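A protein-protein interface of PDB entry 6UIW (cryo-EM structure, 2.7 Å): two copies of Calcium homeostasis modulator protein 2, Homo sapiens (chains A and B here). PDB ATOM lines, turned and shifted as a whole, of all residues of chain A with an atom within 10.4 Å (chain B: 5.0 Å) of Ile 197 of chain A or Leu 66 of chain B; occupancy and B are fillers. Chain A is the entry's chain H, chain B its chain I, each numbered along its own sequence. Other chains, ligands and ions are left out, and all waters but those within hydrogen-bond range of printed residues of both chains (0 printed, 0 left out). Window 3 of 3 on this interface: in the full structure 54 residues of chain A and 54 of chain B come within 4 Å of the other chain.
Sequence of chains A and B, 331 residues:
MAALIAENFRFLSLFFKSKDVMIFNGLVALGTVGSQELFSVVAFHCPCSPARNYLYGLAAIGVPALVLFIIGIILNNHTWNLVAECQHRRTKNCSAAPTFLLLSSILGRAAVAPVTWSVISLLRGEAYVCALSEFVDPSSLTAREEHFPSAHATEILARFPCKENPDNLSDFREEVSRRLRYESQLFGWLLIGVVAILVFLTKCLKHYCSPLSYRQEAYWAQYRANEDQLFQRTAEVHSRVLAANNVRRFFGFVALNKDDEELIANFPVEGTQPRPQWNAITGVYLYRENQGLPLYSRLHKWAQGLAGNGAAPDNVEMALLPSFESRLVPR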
ATOM      1  N   VAL A 115       6.300  15.817 -27.346  1.00  0.00           N
ATOM      2  CA  VAL A 115       7.106  16.760 -26.580  1.00  0.00           C
ATOM      3  C   VAL A 115       7.970  16.019 -25.573  1.00  0.00           C
ATOM      4  O   VAL A 115       9.151  16.336 -25.404  1.00  0.00           O
ATOM      5  CB  VAL A 115       6.194  17.805 -25.913  1.00  0.00           C
ATOM      6  CG1 VAL A 115       6.908  18.525 -24.812  1.00  0.00           C
ATOM      7  CG2 VAL A 115       5.746  18.805 -26.951  1.00  0.00           C
ATOM      8  N   TRP A 189      16.023  21.794 -21.906  1.00  0.00           N
ATOM      9  CA  TRP A 189      15.523  22.402 -20.683  1.00  0.00           C
ATOM     10  C   TRP A 189      14.655  23.613 -20.986  1.00  0.00           C
ATOM     11  O   TRP A 189      13.619  23.794 -20.352  1.00  0.00           O
ATOM     12  CB  TRP A 189      16.673  22.777 -19.751  1.00  0.00           C
ATOM     13  CG  TRP A 189      17.303  21.613 -19.024  1.00  0.00           C
ATOM     14  CD1 TRP A 189      18.606  21.238 -19.075  1.00  0.00           C
ATOM     15  CD2 TRP A 189      16.660  20.685 -18.143  1.00  0.00           C
ATOM     16  NE1 TRP A 189      18.820  20.138 -18.295  1.00  0.00           N
ATOM     17  CE2 TRP A 189      17.640  19.779 -17.707  1.00  0.00           C
ATOM     18  CE3 TRP A 189      15.356  20.536 -17.675  1.00  0.00           C
ATOM     19  CZ2 TRP A 189      17.356  18.740 -16.835  1.00  0.00           C
ATOM     20  CZ3 TRP A 189      15.078  19.503 -16.819  1.00  0.00           C
ATOM     21  CH2 TRP A 189      16.070  18.620 -16.403  1.00  0.00           C
ATOM     22  N   LEU A 190      15.019  24.426 -21.977  1.00  0.00           N
ATOM     23  CA  LEU A 190      14.148  25.543 -22.328  1.00  0.00           C
ATOM     24  C   LEU A 190      12.857  25.059 -22.968  1.00  0.00           C
ATOM     25  O   LEU A 190      11.809  25.690 -22.809  1.00  0.00           O
ATOM     26  CB  LEU A 190      14.867  26.523 -23.247  1.00  0.00           C
ATOM     27  CG  LEU A 190      16.056  27.254 -22.636  1.00  0.00           C
ATOM     28  CD1 LEU A 190      16.583  28.280 -23.612  1.00  0.00           C
ATOM     29  CD2 LEU A 190      15.672  27.901 -21.322  1.00  0.00           C
ATOM     30  N   LEU A 191      12.894  23.896 -23.619  1.00  0.00           N
ATOM     31  CA  LEU A 191      11.674  23.316 -24.162  1.00  0.00           C
ATOM     32  C   LEU A 191      10.751  22.835 -23.061  1.00  0.00           C
ATOM     33  O   LEU A 191       9.555  23.133 -23.084  1.00  0.00           O
ATOM     34  CB  LEU A 191      12.014  22.163 -25.094  1.00  0.00           C
ATOM     35  CG  LEU A 191      10.933  21.907 -26.125  1.00  0.00           C
ATOM     36  CD1 LEU A 191      10.982  23.009 -27.156  1.00  0.00           C
ATOM     37  CD2 LEU A 191      11.151  20.560 -26.757  1.00  0.00           C
ATOM     38  N   ILE A 192      11.282  22.101 -22.083  1.00  0.00           N
ATOM     39  CA  ILE A 192      10.423  21.612 -21.010  1.00  0.00           C
ATOM     40  C   ILE A 192       9.972  22.768 -20.122  1.00  0.00           C
ATOM     41  O   ILE A 192       8.872  22.743 -19.563  1.00  0.00           O
ATOM     42  CB  ILE A 192      11.122  20.484 -20.224  1.00  0.00           C
ATOM     43  CG1 ILE A 192      10.140  19.747 -19.323  1.00  0.00           C
ATOM     44  CG2 ILE A 192      12.232  20.994 -19.378  1.00  0.00           C
ATOM     45  CD1 ILE A 192      10.706  18.468 -18.758  1.00  0.00           C
ATOM     46  N   GLY A 193      10.745  23.855 -20.092  1.00  0.00           N
ATOM     47  CA  GLY A 193      10.320  25.040 -19.373  1.00  0.00           C
ATOM     48  C   GLY A 193       9.157  25.745 -20.040  1.00  0.00           C
ATOM     49  O   GLY A 193       8.170  26.092 -19.386  1.00  0.00           O
ATOM     50  N   VAL A 194       9.251  25.962 -21.359  1.00  0.00           N
ATOM     51  CA  VAL A 194       8.158  26.653 -22.037  1.00  0.00           C
ATOM     52  C   VAL A 194       6.940  25.748 -22.145  1.00  0.00           C
ATOM     53  O   VAL A 194       5.802  26.228 -22.157  1.00  0.00           O
ATOM     54  CB  VAL A 194       8.584  27.199 -23.410  1.00  0.00           C
ATOM     55  CG1 VAL A 194       9.690  28.214 -23.251  1.00  0.00           C
ATOM     56  CG2 VAL A 194       8.971  26.093 -24.372  1.00  0.00           C
ATOM     57  N   VAL A 195       7.146  24.433 -22.145  1.00  0.00           N
ATOM     58  CA  VAL A 195       6.013  23.520 -22.138  1.00  0.00           C
ATOM     59  C   VAL A 195       5.327  23.547 -20.786  1.00  0.00           C
ATOM     60  O   VAL A 195       4.096  23.534 -20.707  1.00  0.00           O
ATOM     61  CB  VAL A 195       6.477  22.110 -22.547  1.00  0.00           C
ATOM     62  CG1 VAL A 195       5.534  21.021 -22.060  1.00  0.00           C
ATOM     63  CG2 VAL A 195       6.581  22.073 -24.042  1.00  0.00           C
ATOM     64  N   ALA A 196       6.101  23.674 -19.706  1.00  0.00           N
ATOM     65  CA  ALA A 196       5.498  23.777 -18.384  1.00  0.00           C
ATOM     66  C   ALA A 196       4.723  25.075 -18.224  1.00  0.00           C
ATOM     67  O   ALA A 196       3.609  25.074 -17.692  1.00  0.00           O
ATOM     68  CB  ALA A 196       6.568  23.657 -17.305  1.00  0.00           C
ATOM     69  N   ILE A 197       5.266  26.191 -18.714  1.00  0.00           N
ATOM     70  CA  ILE A 197       4.539  27.441 -18.520  1.00  0.00           C
ATOM     71  C   ILE A 197       3.357  27.529 -19.474  1.00  0.00           C
ATOM     72  O   ILE A 197       2.357  28.178 -19.167  1.00  0.00           O
ATOM     73  CB  ILE A 197       5.448  28.675 -18.643  1.00  0.00           C
ATOM     74  CG1 ILE A 197       6.009  28.810 -20.042  1.00  0.00           C
ATOM     75  CG2 ILE A 197       6.575  28.602 -17.645  1.00  0.00           C
ATOM     76  CD1 ILE A 197       6.688  30.119 -20.277  1.00  0.00           C
ATOM     77  N   LEU A 198       3.469  26.825 -20.610  1.00  0.00           N
ATOM     78  CA  LEU A 198       2.356  26.702 -21.593  1.00  0.00           C
ATOM     79  C   LEU A 198       1.215  25.890 -20.958  1.00  0.00           C
ATOM     80  O   LEU A 198       0.049  26.307 -21.094  1.00  0.00           O
ATOM     81  CB  LEU A 198       2.881  26.017 -22.857  1.00  0.00           C
ATOM     82  CG  LEU A 198       2.584  26.745 -24.166  1.00  0.00           C
ATOM     83  CD1 LEU A 198       2.857  28.234 -24.031  1.00  0.00           C
ATOM     84  CD2 LEU A 198       3.394  26.155 -25.310  1.00  0.00           C
ATOM     85  N   VAL A 199       1.552  24.778 -20.289  1.00  0.00           N
ATOM     86  CA  VAL A 199       0.586  23.949 -19.573  1.00  0.00           C
ATOM     87  C   VAL A 199      -0.086  24.758 -18.476  1.00  0.00           C
ATOM     88  O   VAL A 199      -1.317  24.728 -18.321  1.00  0.00           O
ATOM     89  CB  VAL A 199       1.278  22.692 -19.020  1.00  0.00           C
ATOM     90  CG1 VAL A 199       0.461  22.051 -17.930  1.00  0.00           C
ATOM     91  CG2 VAL A 199       1.481  21.700 -20.116  1.00  0.00           C
ATOM     92  N   PHE A 200       0.703  25.569 -17.775  1.00  0.00           N
ATOM     93  CA  PHE A 200       0.179  26.423 -16.721  1.00  0.00           C
ATOM     94  C   PHE A 200      -0.772  27.484 -17.264  1.00  0.00           C
ATOM     95  O   PHE A 200      -1.860  27.684 -16.714  1.00  0.00           O
ATOM     96  CB  PHE A 200       1.340  27.070 -15.977  1.00  0.00           C
ATOM     97  CG  PHE A 200       0.921  28.115 -15.008  1.00  0.00           C
ATOM     98  CD1 PHE A 200       0.254  27.773 -13.851  1.00  0.00           C
ATOM     99  CD2 PHE A 200       1.195  29.446 -15.255  1.00  0.00           C
ATOM    100  CE1 PHE A 200      -0.137  28.743 -12.960  1.00  0.00           C
ATOM    101  CE2 PHE A 200       0.804  30.421 -14.369  1.00  0.00           C
ATOM    102  CZ  PHE A 200       0.141  30.065 -13.218  1.00  0.00           C
ATOM    103  N   LEU A 201      -0.407  28.145 -18.363  1.00  0.00           N
ATOM    104  CA  LEU A 201      -1.280  29.186 -18.891  1.00  0.00           C
ATOM    105  C   LEU A 201      -2.502  28.612 -19.587  1.00  0.00           C
ATOM    106  O   LEU A 201      -3.554  29.256 -19.605  1.00  0.00           O
ATOM    107  CB  LEU A 201      -0.528  30.116 -19.834  1.00  0.00           C
ATOM    108  CG  LEU A 201       0.607  30.911 -19.210  1.00  0.00           C
ATOM    109  CD1 LEU A 201       1.344  31.657 -20.295  1.00  0.00           C
ATOM    110  CD2 LEU A 201       0.080  31.855 -18.148  1.00  0.00           C
ATOM    111  N   THR A 202      -2.407  27.405 -20.148  1.00  0.00           N
ATOM    112  CA  THR A 202      -3.601  26.804 -20.725  1.00  0.00           C
ATOM    113  C   THR A 202      -4.577  26.410 -19.638  1.00  0.00           C
ATOM    114  O   THR A 202      -5.786  26.596 -19.794  1.00  0.00           O
ATOM    115  CB  THR A 202      -3.275  25.578 -21.565  1.00  0.00           C
ATOM    116  OG1 THR A 202      -2.284  24.802 -20.892  1.00  0.00           O
ATOM    117  CG2 THR A 202      -2.764  25.993 -22.927  1.00  0.00           C
ATOM    118  N   LYS A 203      -4.069  25.894 -18.515  1.00  0.00           N
ATOM    119  CA  LYS A 203      -4.954  25.573 -17.403  1.00  0.00           C
ATOM    120  C   LYS A 203      -5.568  26.829 -16.806  1.00  0.00           C
ATOM    121  O   LYS A 203      -6.763  26.848 -16.485  1.00  0.00           O
ATOM    122  CB  LYS A 203      -4.200  24.789 -16.339  1.00  0.00           C
ATOM    123  CG  LYS A 203      -4.004  23.341 -16.696  1.00  0.00           C
ATOM    124  CD  LYS A 203      -4.052  22.468 -15.465  1.00  0.00           C
ATOM    125  CE  LYS A 203      -5.393  22.574 -14.761  1.00  0.00           C
ATOM    126  NZ  LYS A 203      -5.508  21.597 -13.640  1.00  0.00           N
ATOM    127  N   CYS A 204      -4.786  27.905 -16.707  1.00  0.00           N
ATOM    128  CA  CYS A 204      -5.311  29.138 -16.133  1.00  0.00           C
ATOM    129  C   CYS A 204      -6.335  29.790 -17.045  1.00  0.00           C
ATOM    130  O   CYS A 204      -7.366  30.275 -16.575  1.00  0.00           O
ATOM    131  CB  CYS A 204      -4.179  30.115 -15.832  1.00  0.00           C
ATOM    132  SG  CYS A 204      -3.225  29.718 -14.370  1.00  0.00           S
ATOM    133  N   LEU A 205      -6.100  29.780 -18.355  1.00  0.00           N
ATOM    134  CA  LEU A 205      -7.069  30.386 -19.257  1.00  0.00           C
ATOM    135  C   LEU A 205      -8.282  29.492 -19.449  1.00  0.00           C
ATOM    136  O   LEU A 205      -9.372  29.983 -19.745  1.00  0.00           O
ATOM    137  CB  LEU A 205      -6.422  30.718 -20.595  1.00  0.00           C
ATOM    138  CG  LEU A 205      -5.390  31.847 -20.564  1.00  0.00           C
ATOM    139  CD1 LEU A 205      -5.107  32.321 -21.975  1.00  0.00           C
ATOM    140  CD2 LEU A 205      -5.833  33.013 -19.682  1.00  0.00           C
ATOM    141  N   GLY B  62      17.483  25.898 -12.509  1.00  0.00           N
ATOM    142  CA  GLY B  62      16.318  26.740 -12.329  1.00  0.00           C
ATOM    143  C   GLY B  62      15.133  26.301 -13.159  1.00  0.00           C
ATOM    144  O   GLY B  62      13.993  26.667 -12.862  1.00  0.00           O
ATOM    145  N   VAL B  63      15.363  25.511 -14.208  1.00  0.00           N
ATOM    146  CA  VAL B  63      14.251  24.990 -14.997  1.00  0.00           C
ATOM    147  C   VAL B  63      13.560  23.816 -14.324  1.00  0.00           C
ATOM    148  O   VAL B  63      12.323  23.797 -14.304  1.00  0.00           O
ATOM    149  CB  VAL B  63      14.701  24.720 -16.436  1.00  0.00           C
ATOM    150  CG1 VAL B  63      13.652  23.965 -17.183  1.00  0.00           C
ATOM    151  CG2 VAL B  63      14.954  26.035 -17.147  1.00  0.00           C
ATOM    152  N   PRO B  64      14.248  22.824 -13.721  1.00  0.00           N
ATOM    153  CA  PRO B  64      13.496  21.898 -12.858  1.00  0.00           C
ATOM    154  C   PRO B  64      12.903  22.571 -11.638  1.00  0.00           C
ATOM    155  O   PRO B  64      11.843  22.149 -11.164  1.00  0.00           O
ATOM    156  CB  PRO B  64      14.540  20.850 -12.472  1.00  0.00           C
ATOM    157  CG  PRO B  64      15.483  20.864 -13.555  1.00  0.00           C
ATOM    158  CD  PRO B  64      15.606  22.294 -13.945  1.00  0.00           C
ATOM    159  N   ALA B  65      13.532  23.643 -11.153  1.00  0.00           N
ATOM    160  CA  ALA B  65      12.919  24.456 -10.109  1.00  0.00           C
ATOM    161  C   ALA B  65      11.633  25.099 -10.599  1.00  0.00           C
ATOM    162  O   ALA B  65      10.606  25.029  -9.923  1.00  0.00           O
ATOM    163  CB  ALA B  65      13.896  25.523  -9.629  1.00  0.00           C
ATOM    164  N   LEU B  66      11.663  25.706 -11.782  1.00  0.00           N
ATOM    165  CA  LEU B  66      10.466  26.356 -12.303  1.00  0.00           C
ATOM    166  C   LEU B  66       9.394  25.338 -12.659  1.00  0.00           C
ATOM    167  O   LEU B  66       8.203  25.612 -12.503  1.00  0.00           O
ATOM    168  CB  LEU B  66      10.832  27.225 -13.502  1.00  0.00           C
ATOM    169  CG  LEU B  66       9.769  28.090 -14.165  1.00  0.00           C
ATOM    170  CD1 LEU B  66      10.377  29.414 -14.550  1.00  0.00           C
ATOM    171  CD2 LEU B  66       9.272  27.405 -15.416  1.00  0.00           C
ATOM    172  N   VAL B  67       9.798  24.151 -13.104  1.00  0.00           N
ATOM    173  CA  VAL B  67       8.839  23.099 -13.418  1.00  0.00           C
ATOM    174  C   VAL B  67       8.159  22.602 -12.155  1.00  0.00           C
ATOM    175  O   VAL B  67       6.932  22.458 -12.114  1.00  0.00           O
ATOM    176  CB  VAL B  67       9.534  21.960 -14.188  1.00  0.00           C
ATOM    177  CG1 VAL B  67       8.738  20.675 -14.119  1.00  0.00           C
ATOM    178  CG2 VAL B  67       9.710  22.356 -15.628  1.00  0.00           C
ATOM    179  N   LEU B  68       8.930  22.370 -11.091  1.00  0.00           N
ATOM    180  CA  LEU B  68       8.334  21.899  -9.848  1.00  0.00           C
ATOM    181  C   LEU B  68       7.497  22.987  -9.191  1.00  0.00           C
ATOM    182  O   LEU B  68       6.480  22.698  -8.553  1.00  0.00           O
ATOM    183  CB  LEU B  68       9.424  21.409  -8.904  1.00  0.00           C
ATOM    184  CG  LEU B  68      10.067  20.092  -9.312  1.00  0.00           C
ATOM    185  CD1 LEU B  68      11.327  19.887  -8.512  1.00  0.00           C
ATOM    186  CD2 LEU B  68       9.101  18.953  -9.105  1.00  0.00           C
ATOM    187  N   PHE B  69       7.879  24.248  -9.386  1.00  0.00           N
ATOM    188  CA  PHE B  69       7.086  25.360  -8.883  1.00  0.00           C
ATOM    189  C   PHE B  69       5.759  25.471  -9.621  1.00  0.00           C
ATOM    190  O   PHE B  69       4.706  25.677  -9.001  1.00  0.00           O
ATOM    191  CB  PHE B  69       7.897  26.643  -9.021  1.00  0.00           C
ATOM    192  CG  PHE B  69       7.205  27.850  -8.508  1.00  0.00           C
ATOM    193  CD1 PHE B  69       6.859  27.947  -7.179  1.00  0.00           C
ATOM    194  CD2 PHE B  69       6.918  28.904  -9.352  1.00  0.00           C
ATOM    195  CE1 PHE B  69       6.229  29.066  -6.700  1.00  0.00           C
ATOM    196  CE2 PHE B  69       6.289  30.029  -8.878  1.00  0.00           C
ATOM    197  CZ  PHE B  69       5.943  30.109  -7.550  1.00  0.00           C
ATOM    198  N   ILE B  70       5.791  25.310 -10.947  1.00  0.00           N
ATOM    199  CA  ILE B  70       4.576  25.325 -11.752  1.00  0.00           C
ATOM    200  C   ILE B  70       3.672  24.163 -11.378  1.00  0.00           C
ATOM    201  O   ILE B  70       2.462  24.340 -11.215  1.00  0.00           O
ATOM    202  CB  ILE B  70       4.942  25.311 -13.247  1.00  0.00           C
ATOM    203  CG1 ILE B  70       5.377  26.703 -13.690  1.00  0.00           C
ATOM    204  CG2 ILE B  70       3.783  24.860 -14.103  1.00  0.00           C
ATOM    205  CD1 ILE B  70       4.399  27.777 -13.343  1.00  0.00           C
ATOM    206  N   ILE B  71       4.254  22.977 -11.190  1.00  0.00           N
ATOM    207  CA  ILE B  71       3.493  21.792 -10.804  1.00  0.00           C
ATOM    208  C   ILE B  71       2.848  21.985  -9.437  1.00  0.00           C
ATOM    209  O   ILE B  71       1.680  21.632  -9.229  1.00  0.00           O
ATOM    210  CB  ILE B  71       4.410  20.557 -10.839  1.00  0.00           C
ATOM    211  CG1 ILE B  71       4.655  20.123 -12.277  1.00  0.00           C
ATOM    212  CG2 ILE B  71       3.827  19.396 -10.077  1.00  0.00           C
ATOM    213  CD1 ILE B  71       5.684  19.041 -12.402  1.00  0.00           C
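Among the printed residues, merely in contact across the chains: Trp 189 of chain A with Val 63 of chain B (3.2 Å), Trp 189 of chain A with Pro 64 of chain B (3.6 Å), Ala 196 of chain A with Ile 70 of chain B (3.6 Å), Ile 197 of chain A with Leu 66 of chain B (3.7 Å), Phe 200 of chain A with Ile 70 of chain B (3.8 Å), Ala 196 of chain A with Val 67 of chain B (3.8 Å) and Ile 192 of chain A with Val 63 of chain B (3.96 Å).
Hydrophobic or aromatic side chains of chain A that line the printed part of chain B: Trp 189, Ile 192, Ala 196, Ile 197 and Phe 200. Among the printed residues, 7 pairs touch across the chains. Among the printed residues, no Asp or Glu carboxylate lies within 4 Å of a Lys or Arg side-chain nitrogen of the other chain.
The backbone carbonyl oxygen (O) of Phe 200 of chain A sits at hydrogen-bond distance from the side-chain sulfur (SG) of Cys 204 of chain A (3.4 Å).
Of the printed residues of chain B, Trp 189 of chain A touches Val 63 (3.2 Å) and Pro 64 (3.6 Å). Of the printed residues of chain B, Ile 192 of chain A touches Val 63 (3.96 Å). Of the printed residues of chain B, Ala 196 of chain A touches Val 67 and Ile 70. Printed residues of chain B within 4 Å of Ile 197 of chain A: Leu 66. Printed residues of chain B within 4 Å of Phe 200 of chain A: Ile 70. Val 63 of chain B touches just these residues of chain A: Trp 189 and Ile 192. Of the printed residues of chain A, Pro 64 of chain B touches Trp 189 (3.6 Å). No residue of chain A comes within 4 Å of Ala 65 of chain B. Leu 66 of chain B touches just one residue of chain A: Ile 197 (3.7 Å). Ile 70 of chain B touches just these residues of chain A: Ala 196 and Phe 200. The nearest residue of chain B that does not touch Ile 197 of chain A is Ile 70 of chain B (4.5 Å). The nearest residue of chain A that does not touch Leu 66 of chain B is Gly 193 of chain A (4.3 Å). The nearest printed residue of chain B that does not touch Ile 192 of chain A is Val 67 of chain B (4.04 Å).
No position is printed for both chains. Of the 7 pairs that touch across the chains among the printed residues, none has its exchanged pair printed and touching as well.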
